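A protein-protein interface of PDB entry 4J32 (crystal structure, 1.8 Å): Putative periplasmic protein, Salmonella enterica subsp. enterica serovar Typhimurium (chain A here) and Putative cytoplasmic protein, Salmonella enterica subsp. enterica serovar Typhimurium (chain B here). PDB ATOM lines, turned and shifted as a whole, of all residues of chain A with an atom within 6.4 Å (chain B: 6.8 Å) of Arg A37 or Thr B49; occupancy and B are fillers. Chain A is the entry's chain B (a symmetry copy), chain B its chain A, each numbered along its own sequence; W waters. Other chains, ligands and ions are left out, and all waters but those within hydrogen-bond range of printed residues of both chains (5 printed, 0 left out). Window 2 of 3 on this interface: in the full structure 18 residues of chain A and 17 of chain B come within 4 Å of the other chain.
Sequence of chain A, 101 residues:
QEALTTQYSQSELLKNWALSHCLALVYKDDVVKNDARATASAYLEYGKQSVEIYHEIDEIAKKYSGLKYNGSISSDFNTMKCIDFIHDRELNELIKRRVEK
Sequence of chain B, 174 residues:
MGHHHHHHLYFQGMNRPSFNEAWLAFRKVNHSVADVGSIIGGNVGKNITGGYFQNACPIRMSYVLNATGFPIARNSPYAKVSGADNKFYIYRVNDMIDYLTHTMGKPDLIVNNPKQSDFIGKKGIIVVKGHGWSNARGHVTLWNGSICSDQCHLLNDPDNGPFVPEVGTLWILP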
ATOM      1  N   TRP A  17       4.597   5.459  17.979  1.00  0.00           N
ATOM      2  CA  TRP A  17       4.599   5.887  16.588  1.00  0.00           C
ATOM      3  C   TRP A  17       3.575   5.107  15.776  1.00  0.00           C
ATOM      4  O   TRP A  17       2.800   5.689  15.026  1.00  0.00           O
ATOM      5  CB  TRP A  17       6.007   5.767  15.948  1.00  0.00           C
ATOM      6  CG  TRP A  17       6.080   6.535  14.645  1.00  0.00           C
ATOM      7  CD1 TRP A  17       6.505   7.817  14.491  1.00  0.00           C
ATOM      8  CD2 TRP A  17       5.673   6.086  13.347  1.00  0.00           C
ATOM      9  NE1 TRP A  17       6.398   8.202  13.182  1.00  0.00           N
ATOM     10  CE2 TRP A  17       5.886   7.161  12.452  1.00  0.00           C
ATOM     11  CE3 TRP A  17       5.165   4.870  12.847  1.00  0.00           C
ATOM     12  CZ2 TRP A  17       5.608   7.070  11.071  1.00  0.00           C
ATOM     13  CZ3 TRP A  17       4.880   4.778  11.484  1.00  0.00           C
ATOM     14  CH2 TRP A  17       5.111   5.869  10.601  1.00  0.00           C
ATOM     15  N   SER A  20      -0.076   6.331  16.677  1.00  0.00           N
ATOM     16  CA  SER A  20      -0.394   7.686  16.222  1.00  0.00           C
ATOM     17  C   SER A  20      -0.409   7.782  14.705  1.00  0.00           C
ATOM     18  O   SER A  20      -1.289   8.451  14.150  1.00  0.00           O
ATOM     19  CB  SER A  20       0.517   8.755  16.843  1.00  0.00           C
ATOM     20  OG  SER A  20       1.865   8.349  16.821  1.00  0.00           O
ATOM     21  N   HIS A  21       0.527   7.100  14.037  1.00  0.00           N
ATOM     22  CA  HIS A  21       0.540   7.089  12.578  1.00  0.00           C
ATOM     23  C   HIS A  21      -0.749   6.471  12.021  1.00  0.00           C
ATOM     24  O   HIS A  21      -1.343   7.003  11.078  1.00  0.00           O
ATOM     25  CB  HIS A  21       1.764   6.348  12.034  1.00  0.00           C
ATOM     26  CG  HIS A  21       1.806   6.298  10.543  1.00  0.00           C
ATOM     27  ND1 HIS A  21       2.061   7.411   9.771  1.00  0.00           N
ATOM     28  CD2 HIS A  21       1.601   5.276   9.682  1.00  0.00           C
ATOM     29  CE1 HIS A  21       2.023   7.071   8.493  1.00  0.00           C
ATOM     30  NE2 HIS A  21       1.724   5.784   8.414  1.00  0.00           N
ATOM     31  N   ALA A  24      -3.529   8.852  12.241  1.00  0.00           N
ATOM     32  CA  ALA A  24      -3.357   9.830  11.166  1.00  0.00           C
ATOM     33  C   ALA A  24      -3.847   9.310   9.818  1.00  0.00           C
ATOM     34  O   ALA A  24      -4.260  10.092   8.965  1.00  0.00           O
ATOM     35  CB  ALA A  24      -1.886  10.245  11.041  1.00  0.00           C
ATOM     36  N   VAL A  32      -7.622  16.712  13.238  1.00  0.00           N
ATOM     37  CA  VAL A  32      -7.264  15.408  13.850  1.00  0.00           C
ATOM     38  C   VAL A  32      -6.071  14.729  13.149  1.00  0.00           C
ATOM     39  O   VAL A  32      -5.128  14.262  13.822  1.00  0.00           O
ATOM     40  CB  VAL A  32      -8.491  14.464  13.916  1.00  0.00           C
ATOM     41  CG1 VAL A  32      -8.072  13.041  14.364  1.00  0.00           C
ATOM     42  CG2 VAL A  32      -9.583  15.074  14.826  1.00  0.00           C
ATOM     43  N   LYS A  33      -6.112  14.642  11.813  1.00  0.00           N
ATOM     44  CA  LYS A  33      -4.997  14.001  11.069  1.00  0.00           C
ATOM     45  C   LYS A  33      -3.685  14.719  11.371  1.00  0.00           C
ATOM     46  O   LYS A  33      -2.681  14.070  11.627  1.00  0.00           O
ATOM     47  CB  LYS A  33      -5.214  14.058   9.539  1.00  0.00           C
ATOM     48  CG  LYS A  33      -6.291  13.126   9.027  1.00  0.00           C
ATOM     49  CD  LYS A  33      -6.523  13.276   7.488  1.00  0.00           C
ATOM     50  CE  LYS A  33      -5.678  12.303   6.691  1.00  0.00           C
ATOM     51  NZ  LYS A  33      -5.936  10.885   7.087  1.00  0.00           N
ATOM     52  N   ASN A  34      -3.698  16.051  11.343  1.00  0.00           N
ATOM     53  CA  ASN A  34      -2.468  16.814  11.587  1.00  0.00           C
ATOM     54  C   ASN A  34      -1.950  16.630  13.010  1.00  0.00           C
ATOM     55  O   ASN A  34      -0.745  16.609  13.244  1.00  0.00           O
ATOM     56  CB  ASN A  34      -2.662  18.301  11.287  1.00  0.00           C
ATOM     57  CG  ASN A  34      -2.678  18.588   9.793  1.00  0.00           C
ATOM     58  OD1 ASN A  34      -1.983  17.916   9.012  1.00  0.00           O
ATOM     59  ND2 ASN A  34      -3.448  19.589   9.396  1.00  0.00           N
ATOM     60  N   ASP A  35      -2.871  16.488  13.950  1.00  0.00           N
ATOM     61  CA  ASP A  35      -2.529  16.271  15.352  1.00  0.00           C
ATOM     62  C   ASP A  35      -1.853  14.908  15.551  1.00  0.00           C
ATOM     63  O   ASP A  35      -0.808  14.801  16.216  1.00  0.00           O
ATOM     64  CB  ASP A  35      -3.808  16.346  16.200  1.00  0.00           C
ATOM     65  CG  ASP A  35      -3.517  16.236  17.691  1.00  0.00           C
ATOM     66  OD1 ASP A  35      -3.539  17.291  18.369  1.00  0.00           O
ATOM     67  OD2 ASP A  35      -3.251  15.100  18.150  1.00  0.00           O
ATOM     68  N   ALA A  36      -2.440  13.868  14.962  1.00  0.00           N
ATOM     69  CA  ALA A  36      -1.862  12.537  15.006  1.00  0.00           C
ATOM     70  C   ALA A  36      -0.493  12.493  14.299  1.00  0.00           C
ATOM     71  O   ALA A  36       0.427  11.856  14.805  1.00  0.00           O
ATOM     72  CB  ALA A  36      -2.843  11.491  14.431  1.00  0.00           C
ATOM     73  N   ARG A  37      -0.352  13.186  13.171  1.00  0.00           N
ATOM     74  CA  ARG A  37       0.947  13.288  12.469  1.00  0.00           C
ATOM     75  C   ARG A  37       1.988  13.995  13.334  1.00  0.00           C
ATOM     76  O   ARG A  37       3.137  13.584  13.392  1.00  0.00           O
ATOM     77  CB  ARG A  37       0.811  14.075  11.178  1.00  0.00           C
ATOM     78  CG  ARG A  37       0.191  13.319  10.070  1.00  0.00           C
ATOM     79  CD  ARG A  37       0.171  14.242   8.848  1.00  0.00           C
ATOM     80  NE  ARG A  37      -0.201  13.492   7.660  1.00  0.00           N
ATOM     81  CZ  ARG A  37       0.023  13.902   6.412  1.00  0.00           C
ATOM     82  NH1 ARG A  37       0.608  15.073   6.179  1.00  0.00           N
ATOM     83  NH2 ARG A  37      -0.343  13.136   5.385  1.00  0.00           N
ATOM     84  N   ALA A  38       1.586  15.081  13.982  1.00  0.00           N
ATOM     85  CA  ALA A  38       2.522  15.849  14.829  1.00  0.00           C
ATOM     86  C   ALA A  38       2.985  14.982  15.991  1.00  0.00           C
ATOM     87  O   ALA A  38       4.187  14.958  16.335  1.00  0.00           O
ATOM     88  CB  ALA A  38       1.857  17.113  15.344  1.00  0.00           C
ATOM     89  N   THR A  39       2.026  14.275  16.594  1.00  0.00           N
ATOM     90  CA  THR A  39       2.287  13.365  17.700  1.00  0.00           C
ATOM     91  C   THR A  39       3.248  12.250  17.253  1.00  0.00           C
ATOM     92  O   THR A  39       4.246  11.965  17.930  1.00  0.00           O
ATOM     93  CB  THR A  39       0.947  12.791  18.253  1.00  0.00           C
ATOM     94  OG1 THR A  39       0.181  13.860  18.829  1.00  0.00           O
ATOM     95  CG2 THR A  39       1.194  11.702  19.320  1.00  0.00           C
ATOM     96  N   ALA A  40       2.969  11.625  16.112  1.00  0.00           N
ATOM     97  CA  ALA A  40       3.898  10.602  15.622  1.00  0.00           C
ATOM     98  C   ALA A  40       5.312  11.183  15.433  1.00  0.00           C
ATOM     99  O   ALA A  40       6.297  10.536  15.787  1.00  0.00           O
ATOM    100  CB  ALA A  40       3.385   9.959  14.318  1.00  0.00           C
ATOM    101  N   SER A  41       5.410  12.417  14.938  1.00  0.00           N
ATOM    102  CA  SER A  41       6.736  12.987  14.646  1.00  0.00           C
ATOM    103  C   SER A  41       7.560  13.130  15.956  1.00  0.00           C
ATOM    104  O   SER A  41       8.795  13.029  15.937  1.00  0.00           O
ATOM    105  CB  SER A  41       6.637  14.315  13.886  1.00  0.00           C
ATOM    106  OG  SER A  41       6.260  15.382  14.726  1.00  0.00           O
ATOM    107  N   ALA A  42       6.873  13.341  17.076  1.00  0.00           N
ATOM    108  CA  ALA A  42       7.542  13.447  18.381  1.00  0.00           C
ATOM    109  C   ALA A  42       8.221  12.117  18.728  1.00  0.00           C
ATOM    110  O   ALA A  42       9.369  12.088  19.208  1.00  0.00           O
ATOM    111  CB  ALA A  42       6.541  13.845  19.472  1.00  0.00           C
ATOM    112  N   ALA B  34       5.472  21.323   4.575  1.00  0.00           N
ATOM    113  CA  ALA B  34       4.982  20.890   3.257  1.00  0.00           C
ATOM    114  C   ALA B  34       5.750  21.600   2.138  1.00  0.00           C
ATOM    115  O   ALA B  34       6.211  20.960   1.189  1.00  0.00           O
ATOM    116  CB  ALA B  34       3.462  21.105   3.088  1.00  0.00           C
ATOM    117  N   GLY B  37       9.350  20.444   1.769  1.00  0.00           N
ATOM    118  CA  GLY B  37       9.361  19.183   1.022  1.00  0.00           C
ATOM    119  C   GLY B  37       9.324  19.418  -0.478  1.00  0.00           C
ATOM    120  O   GLY B  37      10.055  18.771  -1.218  1.00  0.00           O
ATOM    121  N   SER B  38       8.487  20.358  -0.929  1.00  0.00           N
ATOM    122  CA  SER B  38       8.374  20.676  -2.349  1.00  0.00           C
ATOM    123  C   SER B  38       9.668  21.266  -2.887  1.00  0.00           C
ATOM    124  O   SER B  38      10.087  20.964  -4.009  1.00  0.00           O
ATOM    125  CB  SER B  38       7.244  21.670  -2.610  1.00  0.00           C
ATOM    126  OG  SER B  38       5.989  21.089  -2.331  1.00  0.00           O
ATOM    127  N   VAL B  44      13.580  13.655   0.958  1.00  0.00           N
ATOM    128  CA  VAL B  44      13.044  14.687   1.850  1.00  0.00           C
ATOM    129  C   VAL B  44      11.558  14.944   1.518  1.00  0.00           C
ATOM    130  O   VAL B  44      10.678  14.839   2.399  1.00  0.00           O
ATOM    131  CB  VAL B  44      13.882  15.994   1.797  1.00  0.00           C
ATOM    132  CG1 VAL B  44      13.189  17.150   2.558  1.00  0.00           C
ATOM    133  CG2 VAL B  44      15.281  15.759   2.399  1.00  0.00           C
ATOM    134  N   GLY B  45      11.295  15.267   0.260  1.00  0.00           N
ATOM    135  CA  GLY B  45       9.919  15.482  -0.191  1.00  0.00           C
ATOM    136  C   GLY B  45       8.971  14.306   0.009  1.00  0.00           C
ATOM    137  O   GLY B  45       7.836  14.474   0.474  1.00  0.00           O
ATOM    138  N   LYS B  46       9.428  13.109  -0.354  1.00  0.00           N
ATOM    139  CA  LYS B  46       8.637  11.894  -0.179  1.00  0.00           C
ATOM    140  C   LYS B  46       8.233  11.654   1.275  1.00  0.00           C
ATOM    141  O   LYS B  46       7.079  11.308   1.557  1.00  0.00           O
ATOM    142  CB  LYS B  46       9.404  10.695  -0.735  1.00  0.00           C
ATOM    143  CG  LYS B  46       9.456  10.734  -2.263  1.00  0.00           C
ATOM    144  CD  LYS B  46       9.989   9.451  -2.853  1.00  0.00           C
ATOM    145  CE  LYS B  46      10.006   9.548  -4.371  1.00  0.00           C
ATOM    146  NZ  LYS B  46      10.849   8.471  -4.962  1.00  0.00           N
ATOM    147  N   ASN B  47       9.180  11.852   2.195  1.00  0.00           N
ATOM    148  CA  ASN B  47       8.891  11.681   3.614  1.00  0.00           C
ATOM    149  C   ASN B  47       7.979  12.742   4.180  1.00  0.00           C
ATOM    150  O   ASN B  47       7.155  12.450   5.054  1.00  0.00           O
ATOM    151  CB  ASN B  47      10.168  11.567   4.440  1.00  0.00           C
ATOM    152  CG  ASN B  47      10.769  10.179   4.358  1.00  0.00           C
ATOM    153  OD1 ASN B  47      10.276   9.236   4.989  1.00  0.00           O
ATOM    154  ND2 ASN B  47      11.821  10.037   3.558  1.00  0.00           N
ATOM    155  N   ILE B  48       8.119  13.966   3.684  1.00  0.00           N
ATOM    156  CA  ILE B  48       7.197  15.045   4.053  1.00  0.00           C
ATOM    157  C   ILE B  48       5.778  14.834   3.505  1.00  0.00           C
ATOM    158  O   ILE B  48       4.790  14.989   4.236  1.00  0.00           O
ATOM    159  CB  ILE B  48       7.809  16.418   3.715  1.00  0.00           C
ATOM    160  CG1 ILE B  48       8.939  16.723   4.714  1.00  0.00           C
ATOM    161  CG2 ILE B  48       6.745  17.529   3.698  1.00  0.00           C
ATOM    162  CD1 ILE B  48       9.798  17.904   4.266  1.00  0.00           C
ATOM    163  N   THR B  49       5.677  14.426   2.245  1.00  0.00           N
ATOM    164  CA  THR B  49       4.382  14.097   1.650  1.00  0.00           C
ATOM    165  C   THR B  49       3.686  12.972   2.408  1.00  0.00           C
ATOM    166  O   THR B  49       2.461  13.013   2.606  1.00  0.00           O
ATOM    167  CB  THR B  49       4.541  13.757   0.150  1.00  0.00           C
ATOM    168  OG1 THR B  49       5.032  14.922  -0.523  1.00  0.00           O
ATOM    169  CG2 THR B  49       3.216  13.290  -0.489  1.00  0.00           C
ATOM    170  N   GLY B  50       4.466  11.978   2.836  1.00  0.00           N
ATOM    171  CA  GLY B  50       3.942  10.850   3.604  1.00  0.00           C
ATOM    172  C   GLY B  50       3.589  11.213   5.046  1.00  0.00           C
ATOM    173  O   GLY B  50       2.965  10.431   5.760  1.00  0.00           O
ATOM    174  N   GLY B  51       3.979  12.411   5.471  1.00  0.00           N
ATOM    175  CA  GLY B  51       3.736  12.881   6.827  1.00  0.00           C
ATOM    176  C   GLY B  51       4.736  12.438   7.878  1.00  0.00           C
ATOM    177  O   GLY B  51       4.574  12.759   9.069  1.00  0.00           O
ATOM    178  N   TYR B  52       5.799  11.739   7.461  1.00  0.00           N
ATOM    179  CA  TYR B  52       6.766  11.195   8.426  1.00  0.00           C
ATOM    180  C   TYR B  52       7.579  12.286   9.090  1.00  0.00           C
ATOM    181  O   TYR B  52       7.986  12.129  10.240  1.00  0.00           O
ATOM    182  CB  TYR B  52       7.750  10.235   7.754  1.00  0.00           C
ATOM    183  CG  TYR B  52       7.086   9.036   7.138  1.00  0.00           C
ATOM    184  CD1 TYR B  52       6.944   7.859   7.859  1.00  0.00           C
ATOM    185  CD2 TYR B  52       6.612   9.079   5.820  1.00  0.00           C
ATOM    186  CE1 TYR B  52       6.316   6.741   7.295  1.00  0.00           C
ATOM    187  CE2 TYR B  52       5.985   7.968   5.244  1.00  0.00           C
ATOM    188  CZ  TYR B  52       5.850   6.804   6.000  1.00  0.00           C
ATOM    189  OH  TYR B  52       5.254   5.698   5.437  1.00  0.00           O
ATOM    190  N   PHE B  53       7.875  13.359   8.352  1.00  0.00           N
ATOM    191  CA  PHE B  53       8.613  14.483   8.947  1.00  0.00           C
ATOM    192  C   PHE B  53       7.648  15.640   9.062  1.00  0.00           C
ATOM    193  O   PHE B  53       6.971  15.967   8.083  1.00  0.00           O
ATOM    194  CB  PHE B  53       9.768  14.941   8.053  1.00  0.00           C
ATOM    195  CG  PHE B  53      10.791  13.868   7.744  1.00  0.00           C
ATOM    196  CD1 PHE B  53      10.959  12.759   8.579  1.00  0.00           C
ATOM    197  CD2 PHE B  53      11.635  14.028   6.635  1.00  0.00           C
ATOM    198  CE1 PHE B  53      11.930  11.786   8.301  1.00  0.00           C
ATOM    199  CE2 PHE B  53      12.609  13.062   6.343  1.00  0.00           C
ATOM    200  CZ  PHE B  53      12.746  11.939   7.168  1.00  0.00           C
ATOM    201  N   GLN B  54       7.598  16.240  10.254  1.00  0.00           N
ATOM    202  CA  GLN B  54       6.757  17.410  10.512  1.00  0.00           C
ATOM    203  C   GLN B  54       7.552  18.576  11.109  1.00  0.00           C
ATOM    204  O   GLN B  54       7.096  19.725  11.062  1.00  0.00           O
ATOM    205  CB  GLN B  54       5.603  17.027  11.469  1.00  0.00           C
ATOM    206  CG  GLN B  54       4.637  15.993  10.891  1.00  0.00           C
ATOM    207  CD  GLN B  54       3.759  16.580   9.772  1.00  0.00           C
ATOM    208  OE1 GLN B  54       2.717  17.141  10.031  1.00  0.00           O
ATOM    209  NE2 GLN B  54       4.223  16.486   8.532  1.00  0.00           N
HETATM  210  O   HOH W   1       0.852  17.560   8.054  1.00  0.00           O
HETATM  211  O   HOH W   2       1.011  18.208  11.920  1.00  0.00           O
HETATM  212  O   HOH W   3       6.573  10.784  12.161  1.00  0.00           O
HETATM  213  O   HOH W   4       1.137  10.367   8.118  1.00  0.00           O
HETATM  214  O   HOH W   5       3.988  11.792  11.457  1.00  0.00           O
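Arg A37 touches just these residues of chain B: Thr B49, Gly B51 and Gln B54. Printed residues of chain B within 4 Å of Trp A17: Tyr B52. Printed residues of chain B within 4 Å of Ser A41: Gln B54. Of the printed residues of chain A, Gly B51 touches Arg A37 (3.9 Å). The nearest residue of chain B that does not touch Arg A37 is Gly B50 (4.3 Å).
Water W5 lies within hydrogen-bond range of O of Gly B51 (2.6 Å) and O of Arg A37 (2.8 Å). Water W2 lies within hydrogen-bond range of the backbone carbonyl oxygen (O) of Asn A34 (2.7 Å) and the side-chain amide oxygen (OE1) of Gln B54 (2.8 Å). Water W3 lies within hydrogen-bond range of O of Tyr B52 (2.7 Å), NE1 of Trp A17 (2.8 Å) and N of Ser A41 (3.4 Å). Water W1 lies within hydrogen-bond range of OE1 of Gln B54, OD1 of Asn A34 and NH1 of Arg A37. Water W4 bridges O of Gly B50 (3.0 Å) and NE of Arg A37 (3.4 Å).
Of the 14 printed residues of chain B, 4 touch a printed residue of chain A. Hydrophobic or aromatic side chains of chain B that line the printed part of chain A: Tyr B52. Along chain B the printed residues that touch a printed residue of chain A span positions 49 to 54. Of the 15 printed residues of chain A, 3 touch a printed residue of chain B. Printed residues of chain A that touch a printed residue of chain B: Trp A17, Arg A37 and Ser A41. Among the printed residues, no Asp or Glu carboxylate lies within 4 Å of a Lys or Arg side-chain nitrogen of the other chain.
Trp A17 touches Tyr B52. NH2 of Arg A37 touches O of Thr B49, at 3.9 Å. CA of Gly B51 touches CZ of Arg A37, at 3.9 Å. Gln B54 touches Arg A37. Ser A41 touches Gln B54.
O of Ala A38 sits at hydrogen-bond distance from OG of Ser A41 (2.7 Å). The side-chain hydroxyl of Ser A20 is in hydrogen-bond range of the backbone carbonyl oxygen of Trp A17 (3.3 Å). The backbone carbonyl oxygen of Ala A40 lies close to the indole nitrogen of Trp A17 (3.5 Å). OG1 of Thr B49 is in hydrogen-bond range of O of Gly B45 (3.0 Å). O of Asn B47 sits at hydrogen-bond distance from N of Tyr B52 (2.9 Å).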
